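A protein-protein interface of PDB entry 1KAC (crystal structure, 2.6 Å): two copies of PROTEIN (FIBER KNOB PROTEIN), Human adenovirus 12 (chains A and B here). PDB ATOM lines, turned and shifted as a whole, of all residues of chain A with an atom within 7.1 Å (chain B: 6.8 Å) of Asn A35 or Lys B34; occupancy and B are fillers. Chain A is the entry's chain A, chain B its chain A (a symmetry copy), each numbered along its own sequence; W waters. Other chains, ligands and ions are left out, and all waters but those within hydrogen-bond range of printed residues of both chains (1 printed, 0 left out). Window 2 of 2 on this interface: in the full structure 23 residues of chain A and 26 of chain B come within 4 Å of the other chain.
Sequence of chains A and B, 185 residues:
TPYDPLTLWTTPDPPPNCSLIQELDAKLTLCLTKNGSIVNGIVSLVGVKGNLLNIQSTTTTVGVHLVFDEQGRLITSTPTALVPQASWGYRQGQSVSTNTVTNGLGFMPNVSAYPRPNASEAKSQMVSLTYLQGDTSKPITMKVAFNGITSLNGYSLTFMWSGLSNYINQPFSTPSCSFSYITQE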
ATOM      1  N   LEU A   6      -2.208 -19.489 -22.129  1.00  0.00           N
ATOM      2  CA  LEU A   6      -0.931 -19.644 -21.450  1.00  0.00           C
ATOM      3  C   LEU A   6       0.006 -20.583 -22.185  1.00  0.00           C
ATOM      4  O   LEU A   6       1.126 -20.835 -21.738  1.00  0.00           O
ATOM      5  CB  LEU A   6      -1.147 -20.156 -20.031  1.00  0.00           C
ATOM      6  CG  LEU A   6      -1.948 -19.230 -19.122  1.00  0.00           C
ATOM      7  CD1 LEU A   6      -1.976 -19.810 -17.718  1.00  0.00           C
ATOM      8  CD2 LEU A   6      -1.313 -17.846 -19.116  1.00  0.00           C
ATOM      9  N   THR A  33       4.927 -22.648 -22.352  1.00  0.00           N
ATOM     10  CA  THR A  33       3.859 -22.370 -21.402  1.00  0.00           C
ATOM     11  C   THR A  33       4.317 -21.271 -20.448  1.00  0.00           C
ATOM     12  O   THR A  33       5.413 -21.329 -19.886  1.00  0.00           O
ATOM     13  CB  THR A  33       3.448 -23.633 -20.611  1.00  0.00           C
ATOM     14  OG1 THR A  33       4.594 -24.200 -19.960  1.00  0.00           O
ATOM     15  CG2 THR A  33       2.832 -24.658 -21.551  1.00  0.00           C
ATOM     16  N   LYS A  34       3.475 -20.255 -20.294  1.00  0.00           N
ATOM     17  CA  LYS A  34       3.800 -19.140 -19.433  1.00  0.00           C
ATOM     18  C   LYS A  34       3.401 -19.353 -17.983  1.00  0.00           C
ATOM     19  O   LYS A  34       2.226 -19.537 -17.659  1.00  0.00           O
ATOM     20  CB  LYS A  34       3.137 -17.862 -19.941  1.00  0.00           C
ATOM     21  CG  LYS A  34       3.463 -16.648 -19.076  1.00  0.00           C
ATOM     22  CD  LYS A  34       2.790 -15.386 -19.575  1.00  0.00           C
ATOM     23  CE  LYS A  34       3.242 -14.186 -18.771  1.00  0.00           C
ATOM     24  NZ  LYS A  34       4.709 -14.003 -18.881  1.00  0.00           N
ATOM     25  N   ASN A  35       4.401 -19.326 -17.115  1.00  0.00           N
ATOM     26  CA  ASN A  35       4.190 -19.465 -15.682  1.00  0.00           C
ATOM     27  C   ASN A  35       4.741 -18.196 -15.042  1.00  0.00           C
ATOM     28  O   ASN A  35       5.880 -18.173 -14.578  1.00  0.00           O
ATOM     29  CB  ASN A  35       4.936 -20.688 -15.138  1.00  0.00           C
ATOM     30  CG  ASN A  35       4.857 -20.782 -13.627  1.00  0.00           C
ATOM     31  OD1 ASN A  35       3.784 -20.603 -13.048  1.00  0.00           O
ATOM     32  ND2 ASN A  35       5.987 -21.074 -12.982  1.00  0.00           N
ATOM     33  N   GLY A  36       3.939 -17.138 -15.036  1.00  0.00           N
ATOM     34  CA  GLY A  36       4.399 -15.887 -14.468  1.00  0.00           C
ATOM     35  C   GLY A  36       5.517 -15.299 -15.307  1.00  0.00           C
ATOM     36  O   GLY A  36       5.382 -15.178 -16.520  1.00  0.00           O
ATOM     37  N   SER A  37       6.627 -14.944 -14.670  1.00  0.00           N
ATOM     38  CA  SER A  37       7.758 -14.361 -15.382  1.00  0.00           C
ATOM     39  C   SER A  37       8.654 -15.373 -16.071  1.00  0.00           C
ATOM     40  O   SER A  37       9.652 -14.996 -16.696  1.00  0.00           O
ATOM     41  CB  SER A  37       8.604 -13.517 -14.439  1.00  0.00           C
ATOM     42  OG  SER A  37       7.848 -12.427 -13.969  1.00  0.00           O
ATOM     43  N   ILE A  38       8.320 -16.654 -15.949  1.00  0.00           N
ATOM     44  CA  ILE A  38       9.115 -17.682 -16.599  1.00  0.00           C
ATOM     45  C   ILE A  38       8.314 -18.540 -17.567  1.00  0.00           C
ATOM     46  O   ILE A  38       7.189 -18.942 -17.281  1.00  0.00           O
ATOM     47  CB  ILE A  38       9.795 -18.626 -15.585  1.00  0.00           C
ATOM     48  CG1 ILE A  38      10.801 -17.849 -14.731  1.00  0.00           C
ATOM     49  CG2 ILE A  38      10.525 -19.738 -16.329  1.00  0.00           C
ATOM     50  CD1 ILE A  38      11.541 -18.700 -13.692  1.00  0.00           C
ATOM     51  N   VAL A  39       8.900 -18.791 -18.730  1.00  0.00           N
ATOM     52  CA  VAL A  39       8.290 -19.661 -19.723  1.00  0.00           C
ATOM     53  C   VAL A  39       8.963 -21.025 -19.595  1.00  0.00           C
ATOM     54  O   VAL A  39      10.191 -21.121 -19.527  1.00  0.00           O
ATOM     55  CB  VAL A  39       8.504 -19.150 -21.171  1.00  0.00           C
ATOM     56  CG1 VAL A  39       8.289 -20.288 -22.172  1.00  0.00           C
ATOM     57  CG2 VAL A  39       7.524 -18.025 -21.473  1.00  0.00           C
ATOM     58  N   ASN A  40       8.156 -22.074 -19.510  1.00  0.00           N
ATOM     59  CA  ASN A  40       8.698 -23.419 -19.457  1.00  0.00           C
ATOM     60  C   ASN A  40       8.591 -23.865 -20.894  1.00  0.00           C
ATOM     61  O   ASN A  40       7.517 -23.795 -21.488  1.00  0.00           O
ATOM     62  CB  ASN A  40       7.853 -24.323 -18.566  1.00  0.00           C
ATOM     63  CG  ASN A  40       7.993 -23.985 -17.100  1.00  0.00           C
ATOM     64  OD1 ASN A  40       9.086 -24.067 -16.544  1.00  0.00           O
ATOM     65  ND2 ASN A  40       6.891 -23.600 -16.466  1.00  0.00           N
ATOM     66  N   GLY A 106       4.136 -11.960 -23.436  1.00  0.00           N
ATOM     67  CA  GLY A 106       4.189 -12.758 -22.224  1.00  0.00           C
ATOM     68  C   GLY A 106       5.034 -14.007 -22.438  1.00  0.00           C
ATOM     69  O   GLY A 106       5.469 -14.654 -21.478  1.00  0.00           O
ATOM     70  N   THR A 183      10.365 -13.766 -18.960  1.00  0.00           N
ATOM     71  CA  THR A 183       9.540 -13.184 -20.000  1.00  0.00           C
ATOM     72  C   THR A 183       9.578 -11.661 -20.062  1.00  0.00           C
ATOM     73  O   THR A 183       9.778 -10.983 -19.054  1.00  0.00           O
ATOM     74  CB  THR A 183       8.067 -13.650 -19.863  1.00  0.00           C
ATOM     75  OG1 THR A 183       7.489 -13.088 -18.676  1.00  0.00           O
ATOM     76  CG2 THR A 183       8.003 -15.173 -19.780  1.00  0.00           C
ATOM     77  N   ASP B   4       3.152  -8.931  -9.697  1.00  0.00           N
ATOM     78  CA  ASP B   4       2.821 -10.340  -9.852  1.00  0.00           C
ATOM     79  C   ASP B   4       3.237 -11.114  -8.607  1.00  0.00           C
ATOM     80  O   ASP B   4       4.421 -11.259  -8.315  1.00  0.00           O
ATOM     81  CB  ASP B   4       3.491 -10.928 -11.094  1.00  0.00           C
ATOM     82  CG  ASP B   4       3.304 -12.434 -11.194  1.00  0.00           C
ATOM     83  OD1 ASP B   4       2.277 -12.939 -10.693  1.00  0.00           O
ATOM     84  OD2 ASP B   4       4.172 -13.108 -11.793  1.00  0.00           O
ATOM     85  N   PRO B   5       2.253 -11.604  -7.845  1.00  0.00           N
ATOM     86  CA  PRO B   5       2.432 -12.372  -6.606  1.00  0.00           C
ATOM     87  C   PRO B   5       3.011 -13.770  -6.812  1.00  0.00           C
ATOM     88  O   PRO B   5       3.361 -14.449  -5.849  1.00  0.00           O
ATOM     89  CB  PRO B   5       1.015 -12.417  -6.037  1.00  0.00           C
ATOM     90  CG  PRO B   5       0.186 -12.546  -7.324  1.00  0.00           C
ATOM     91  CD  PRO B   5       0.816 -11.410  -8.121  1.00  0.00           C
ATOM     92  N   LEU B   6       3.108 -14.198  -8.065  1.00  0.00           N
ATOM     93  CA  LEU B   6       3.648 -15.515  -8.364  1.00  0.00           C
ATOM     94  C   LEU B   6       5.112 -15.465  -8.759  1.00  0.00           C
ATOM     95  O   LEU B   6       5.721 -16.493  -9.056  1.00  0.00           O
ATOM     96  CB  LEU B   6       2.847 -16.173  -9.481  1.00  0.00           C
ATOM     97  CG  LEU B   6       1.378 -16.432  -9.161  1.00  0.00           C
ATOM     98  CD1 LEU B   6       0.744 -17.196 -10.309  1.00  0.00           C
ATOM     99  CD2 LEU B   6       1.271 -17.225  -7.865  1.00  0.00           C
ATOM    100  N   THR B   7       5.680 -14.265  -8.754  1.00  0.00           N
ATOM    101  CA  THR B   7       7.077 -14.101  -9.120  1.00  0.00           C
ATOM    102  C   THR B   7       7.884 -13.270  -8.134  1.00  0.00           C
ATOM    103  O   THR B   7       7.431 -12.236  -7.653  1.00  0.00           O
ATOM    104  CB  THR B   7       7.214 -13.442 -10.504  1.00  0.00           C
ATOM    105  OG1 THR B   7       6.631 -14.290 -11.498  1.00  0.00           O
ATOM    106  CG2 THR B   7       8.675 -13.202 -10.836  1.00  0.00           C
ATOM    107  N   LEU B   8       9.082 -13.749  -7.832  1.00  0.00           N
ATOM    108  CA  LEU B   8      10.006 -13.044  -6.954  1.00  0.00           C
ATOM    109  C   LEU B   8      11.290 -12.998  -7.756  1.00  0.00           C
ATOM    110  O   LEU B   8      11.786 -14.042  -8.179  1.00  0.00           O
ATOM    111  CB  LEU B   8      10.275 -13.810  -5.656  1.00  0.00           C
ATOM    112  CG  LEU B   8       9.172 -14.037  -4.627  1.00  0.00           C
ATOM    113  CD1 LEU B   8       9.782 -14.750  -3.427  1.00  0.00           C
ATOM    114  CD2 LEU B   8       8.554 -12.706  -4.195  1.00  0.00           C
ATOM    115  N   LEU B  32      12.264 -16.356  -9.525  1.00  0.00           N
ATOM    116  CA  LEU B  32      11.530 -17.508  -9.010  1.00  0.00           C
ATOM    117  C   LEU B  32      10.042 -17.345  -9.312  1.00  0.00           C
ATOM    118  O   LEU B  32       9.441 -16.320  -8.976  1.00  0.00           O
ATOM    119  CB  LEU B  32      11.702 -17.624  -7.492  1.00  0.00           C
ATOM    120  CG  LEU B  32      13.107 -17.738  -6.902  1.00  0.00           C
ATOM    121  CD1 LEU B  32      12.998 -17.744  -5.375  1.00  0.00           C
ATOM    122  CD2 LEU B  32      13.803 -19.001  -7.414  1.00  0.00           C
ATOM    123  N   THR B  33       9.447 -18.342  -9.956  1.00  0.00           N
ATOM    124  CA  THR B  33       8.024 -18.279 -10.259  1.00  0.00           C
ATOM    125  C   THR B  33       7.336 -19.504  -9.662  1.00  0.00           C
ATOM    126  O   THR B  33       7.782 -20.639  -9.843  1.00  0.00           O
ATOM    127  CB  THR B  33       7.760 -18.200 -11.780  1.00  0.00           C
ATOM    128  OG1 THR B  33       8.390 -19.305 -12.446  1.00  0.00           O
ATOM    129  CG2 THR B  33       8.301 -16.891 -12.334  1.00  0.00           C
ATOM    130  N   LYS B  34       6.257 -19.257  -8.928  1.00  0.00           N
ATOM    131  CA  LYS B  34       5.526 -20.329  -8.291  1.00  0.00           C
ATOM    132  C   LYS B  34       4.461 -20.951  -9.177  1.00  0.00           C
ATOM    133  O   LYS B  34       3.522 -20.285  -9.619  1.00  0.00           O
ATOM    134  CB  LYS B  34       4.866 -19.836  -7.005  1.00  0.00           C
ATOM    135  CG  LYS B  34       4.094 -20.936  -6.282  1.00  0.00           C
ATOM    136  CD  LYS B  34       3.429 -20.438  -5.016  1.00  0.00           C
ATOM    137  CE  LYS B  34       2.786 -21.584  -4.264  1.00  0.00           C
ATOM    138  NZ  LYS B  34       3.801 -22.598  -3.886  1.00  0.00           N
ATOM    139  N   ASN B  35       4.623 -22.241  -9.431  1.00  0.00           N
ATOM    140  CA  ASN B  35       3.670 -23.003 -10.223  1.00  0.00           C
ATOM    141  C   ASN B  35       3.168 -24.128  -9.325  1.00  0.00           C
ATOM    142  O   ASN B  35       3.672 -25.248  -9.384  1.00  0.00           O
ATOM    143  CB  ASN B  35       4.344 -23.592 -11.467  1.00  0.00           C
ATOM    144  CG  ASN B  35       3.418 -24.511 -12.239  1.00  0.00           C
ATOM    145  OD1 ASN B  35       2.253 -24.176 -12.462  1.00  0.00           O
ATOM    146  ND2 ASN B  35       3.930 -25.668 -12.661  1.00  0.00           N
ATOM    147  N   GLY B  36       2.190 -23.821  -8.482  1.00  0.00           N
ATOM    148  CA  GLY B  36       1.675 -24.829  -7.577  1.00  0.00           C
ATOM    149  C   GLY B  36       2.725 -25.213  -6.552  1.00  0.00           C
ATOM    150  O   GLY B  36       3.313 -24.346  -5.914  1.00  0.00           O
ATOM    151  N   SER B  37       2.974 -26.509  -6.399  1.00  0.00           N
ATOM    152  CA  SER B  37       3.958 -26.984  -5.434  1.00  0.00           C
ATOM    153  C   SER B  37       5.395 -26.917  -5.919  1.00  0.00           C
ATOM    154  O   SER B  37       6.315 -27.306  -5.191  1.00  0.00           O
ATOM    155  CB  SER B  37       3.647 -28.415  -5.015  1.00  0.00           C
ATOM    156  OG  SER B  37       2.409 -28.455  -4.347  1.00  0.00           O
ATOM    157  N   ILE B  38       5.594 -26.447  -7.146  1.00  0.00           N
ATOM    158  CA  ILE B  38       6.942 -26.331  -7.674  1.00  0.00           C
ATOM    159  C   ILE B  38       7.306 -24.913  -8.089  1.00  0.00           C
ATOM    160  O   ILE B  38       6.510 -24.205  -8.701  1.00  0.00           O
ATOM    161  CB  ILE B  38       7.177 -27.252  -8.890  1.00  0.00           C
ATOM    162  CG1 ILE B  38       7.057 -28.720  -8.473  1.00  0.00           C
ATOM    163  CG2 ILE B  38       8.571 -27.006  -9.457  1.00  0.00           C
ATOM    164  CD1 ILE B  38       7.283 -29.723  -9.610  1.00  0.00           C
ATOM    165  N   VAL B  39       8.511 -24.500  -7.722  1.00  0.00           N
ATOM    166  CA  VAL B  39       9.026 -23.197  -8.114  1.00  0.00           C
ATOM    167  C   VAL B  39       9.956 -23.425  -9.304  1.00  0.00           C
ATOM    168  O   VAL B  39      10.806 -24.319  -9.281  1.00  0.00           O
ATOM    169  CB  VAL B  39       9.845 -22.518  -6.985  1.00  0.00           C
ATOM    170  CG1 VAL B  39      10.745 -21.426  -7.567  1.00  0.00           C
ATOM    171  CG2 VAL B  39       8.901 -21.899  -5.964  1.00  0.00           C
ATOM    172  N   ASN B  40       9.757 -22.652 -10.362  1.00  0.00           N
ATOM    173  CA  ASN B  40      10.632 -22.742 -11.516  1.00  0.00           C
ATOM    174  C   ASN B  40      11.597 -21.608 -11.277  1.00  0.00           C
ATOM    175  O   ASN B  40      11.180 -20.470 -11.068  1.00  0.00           O
ATOM    176  CB  ASN B  40       9.866 -22.508 -12.814  1.00  0.00           C
ATOM    177  CG  ASN B  40       8.949 -23.659 -13.159  1.00  0.00           C
ATOM    178  OD1 ASN B  40       9.406 -24.782 -13.358  1.00  0.00           O
ATOM    179  ND2 ASN B  40       7.650 -23.390 -13.227  1.00  0.00           N
ATOM    180  N   ASN B 103       3.341 -13.881   0.950  1.00  0.00           N
ATOM    181  CA  ASN B 103       3.101 -15.274   0.585  1.00  0.00           C
ATOM    182  C   ASN B 103       4.452 -15.948   0.363  1.00  0.00           C
ATOM    183  O   ASN B 103       4.576 -16.869  -0.441  1.00  0.00           O
ATOM    184  CB  ASN B 103       2.264 -15.351  -0.694  1.00  0.00           C
ATOM    185  CG  ASN B 103       2.987 -14.782  -1.897  1.00  0.00           C
ATOM    186  OD1 ASN B 103       4.081 -14.228  -1.775  1.00  0.00           O
ATOM    187  ND2 ASN B 103       2.376 -14.908  -3.068  1.00  0.00           N
ATOM    188  N   LEU B 105       6.230 -18.148   1.960  1.00  0.00           N
ATOM    189  CA  LEU B 105       6.380 -19.588   2.104  1.00  0.00           C
ATOM    190  C   LEU B 105       5.989 -20.360   0.848  1.00  0.00           C
ATOM    191  O   LEU B 105       6.290 -21.547   0.729  1.00  0.00           O
ATOM    192  CB  LEU B 105       5.600 -20.092   3.316  1.00  0.00           C
ATOM    193  CG  LEU B 105       6.161 -19.592   4.654  1.00  0.00           C
ATOM    194  CD1 LEU B 105       5.393 -20.243   5.791  1.00  0.00           C
ATOM    195  CD2 LEU B 105       7.639 -19.936   4.771  1.00  0.00           C
ATOM    196  N   GLY B 106       5.334 -19.684  -0.091  1.00  0.00           N
ATOM    197  CA  GLY B 106       4.957 -20.326  -1.338  1.00  0.00           C
ATOM    198  C   GLY B 106       6.166 -20.478  -2.252  1.00  0.00           C
ATOM    199  O   GLY B 106       6.146 -21.262  -3.208  1.00  0.00           O
ATOM    200  N   PHE B 107       7.226 -19.725  -1.953  1.00  0.00           N
ATOM    201  CA  PHE B 107       8.450 -19.790  -2.744  1.00  0.00           C
ATOM    202  C   PHE B 107       9.592 -20.507  -2.022  1.00  0.00           C
ATOM    203  O   PHE B 107      10.636 -20.773  -2.619  1.00  0.00           O
ATOM    204  CB  PHE B 107       8.946 -18.394  -3.119  1.00  0.00           C
ATOM    205  CG  PHE B 107       7.922 -17.533  -3.795  1.00  0.00           C
ATOM    206  CD1 PHE B 107       6.967 -16.853  -3.052  1.00  0.00           C
ATOM    207  CD2 PHE B 107       7.948 -17.360  -5.174  1.00  0.00           C
ATOM    208  CE1 PHE B 107       6.056 -16.005  -3.676  1.00  0.00           C
ATOM    209  CE2 PHE B 107       7.039 -16.514  -5.803  1.00  0.00           C
ATOM    210  CZ  PHE B 107       6.095 -15.836  -5.056  1.00  0.00           C
ATOM    211  N   MET B 108       9.410 -20.814  -0.742  1.00  0.00           N
ATOM    212  CA  MET B 108      10.460 -21.487   0.023  1.00  0.00           C
ATOM    213  C   MET B 108      10.543 -22.992  -0.232  1.00  0.00           C
ATOM    214  O   MET B 108       9.541 -23.645  -0.505  1.00  0.00           O
ATOM    215  CB  MET B 108      10.253 -21.242   1.518  1.00  0.00           C
ATOM    216  CG  MET B 108      10.332 -19.784   1.928  1.00  0.00           C
ATOM    217  SD  MET B 108      11.892 -19.006   1.448  1.00  0.00           S
ATOM    218  CE  MET B 108      11.505 -18.262  -0.141  1.00  0.00           C
ATOM    219  N   THR B 183       7.686 -26.618  -3.001  1.00  0.00           N
ATOM    220  CA  THR B 183       7.509 -25.488  -2.111  1.00  0.00           C
ATOM    221  C   THR B 183       6.972 -25.848  -0.730  1.00  0.00           C
ATOM    222  O   THR B 183       6.238 -26.822  -0.560  1.00  0.00           O
ATOM    223  CB  THR B 183       6.586 -24.419  -2.752  1.00  0.00           C
ATOM    224  OG1 THR B 183       5.249 -24.931  -2.854  1.00  0.00           O
ATOM    225  CG2 THR B 183       7.092 -24.055  -4.145  1.00  0.00           C
ATOM    226  N   GLN B 184       7.365 -25.045   0.255  1.00  0.00           N
ATOM    227  CA  GLN B 184       6.937 -25.226   1.630  1.00  0.00           C
ATOM    228  C   GLN B 184       5.417 -25.189   1.675  1.00  0.00           C
ATOM    229  O   GLN B 184       4.781 -26.070   2.251  1.00  0.00           O
ATOM    230  CB  GLN B 184       7.516 -24.109   2.497  1.00  0.00           C
ATOM    231  CG  GLN B 184       7.141 -24.198   3.959  1.00  0.00           C
ATOM    232  CD  GLN B 184       7.316 -25.604   4.509  1.00  0.00           C
ATOM    233  OE1 GLN B 184       8.293 -26.293   4.200  1.00  0.00           O
ATOM    234  NE2 GLN B 184       6.377 -26.029   5.339  1.00  0.00           N
ATOM    235  N   GLU B 185       4.849 -24.162   1.053  1.00  0.00           N
ATOM    236  CA  GLU B 185       3.409 -23.982   0.986  1.00  0.00           C
ATOM    237  C   GLU B 185       2.939 -23.801  -0.450  1.00  0.00           C
ATOM    238  O   GLU B 185       1.865 -24.325  -0.790  1.00  0.00           O
ATOM    239  CB  GLU B 185       2.975 -22.796   1.845  1.00  0.00           C
ATOM    240  CG  GLU B 185       3.211 -23.037   3.323  1.00  0.00           C
ATOM    241  CD  GLU B 185       2.514 -22.029   4.222  1.00  0.00           C
ATOM    242  OE1 GLU B 185       2.581 -22.210   5.460  1.00  0.00           O
ATOM    243  OE2 GLU B 185       1.904 -21.065   3.702  1.00  0.00           O
ATOM    244  OXT GLU B 185       3.635 -23.118  -1.221  1.00  0.00           O
HETATM  245  O   HOH W   1       5.312 -11.765 -14.019  1.00  0.00           O
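Thr A33 touches none of the printed residues of chain B.
Asn A35 touches four residues of chain B.
Of the printed residues of chain B, Ser A37 touches Thr B7 (3.2 Å) and Thr B33 (3.5 Å).
Of the printed residues of chain B, Ile A38 touches Thr B33 and Asn B40.
Printed residues of chain B within 4 Å of Asn A40: Asn B40.
Printed residues of chain A within 4 Å of Asp B4: Gly A36.
Lys B34 touches just one residue of chain A: Asn A35.
The nearest residue of chain B that does not touch Asn A35 is Thr B7 (5.0 Å).
The side-chain amide nitrogen (ND2) of Asn A35 sits close to the side-chain amide nitrogen (ND2) of Asn B40, 2.9 Å away.
O of Lys B34 sits close to OD1 of Asn A35 (3.5 Å).
The side-chain amide nitrogen (ND2) of Asn A35 is in hydrogen-bond range of the side-chain hydroxyl (OG1) of Thr B33 (3.0 Å).
The side-chain amide oxygen (OD1) of Asn A40 lies close to the side-chain amide oxygen (OD1) of Asn B40, at 3.3 Å.
The side-chain hydroxyl of Thr B7 lies within hydrogen-bond range of the backbone NH of Ser A37 (3.2 Å).
Among the printed residues, pairs that only touch across the chains: Asn A35 with Asn B35, Gly A36 with Asp B4, Ser A37 with Thr B33, Ile A38 with Thr B33 and Ile A38 with Asn B40.
Of the 22 printed residues of chain B, 6 touch a printed residue of chain A.
Among the printed residues, 10 pairs touch across the chains.
Among the printed residues, no Asp or Glu carboxylate lies within 4 Å of a Lys or Arg side-chain nitrogen of the other chain.
The side-chain carboxylate (OD2) of Asp B4 sits at hydrogen-bond distance from the side-chain hydroxyl (OG1) of Thr B7 (2.7 Å).
The backbone NH (N) of Thr A183 is in hydrogen-bond range of the backbone carbonyl oxygen (O) of Ser A37, at 2.7 Å.
The side-chain amino group of Lys B34 is in hydrogen-bond range of the backbone carbonyl oxygen of Gly B36, 2.7 Å away.
The backbone NH (N) of Lys B34 lies within hydrogen-bond range of the backbone carbonyl oxygen (O) of Leu B6 (2.8 Å).
NZ of Lys B34 lies within hydrogen-bond range of OG1 of Thr B183, at 2.9 Å.
The side-chain amino group (NZ) of Lys B34 is in salt-bridge range of the chain-end carboxylate (OXT) of Glu B185.
Asn A35 touches Thr B33, but with the chains exchanged Thr A33 does not touch Asn B35 (7.5 Å).
Asn A35 touches Asn B40, but with the chains exchanged Asn A40 does not touch Asn B35 (5.2 Å).
Ile A38 touches Thr B33, but with the chains exchanged Thr A33 does not touch Ile B38 (11.4 Å).
Asn A40 touches its own counterpart, Asn B40.
Of the 10 pairs that touch across the chains among the printed residues, 2 have their exchanged pair printed and touching as well.
Water W1 lies within hydrogen-bond range of OG of Ser A37 (2.6 Å) and OD2 of Asp B4 (2.8 Å).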
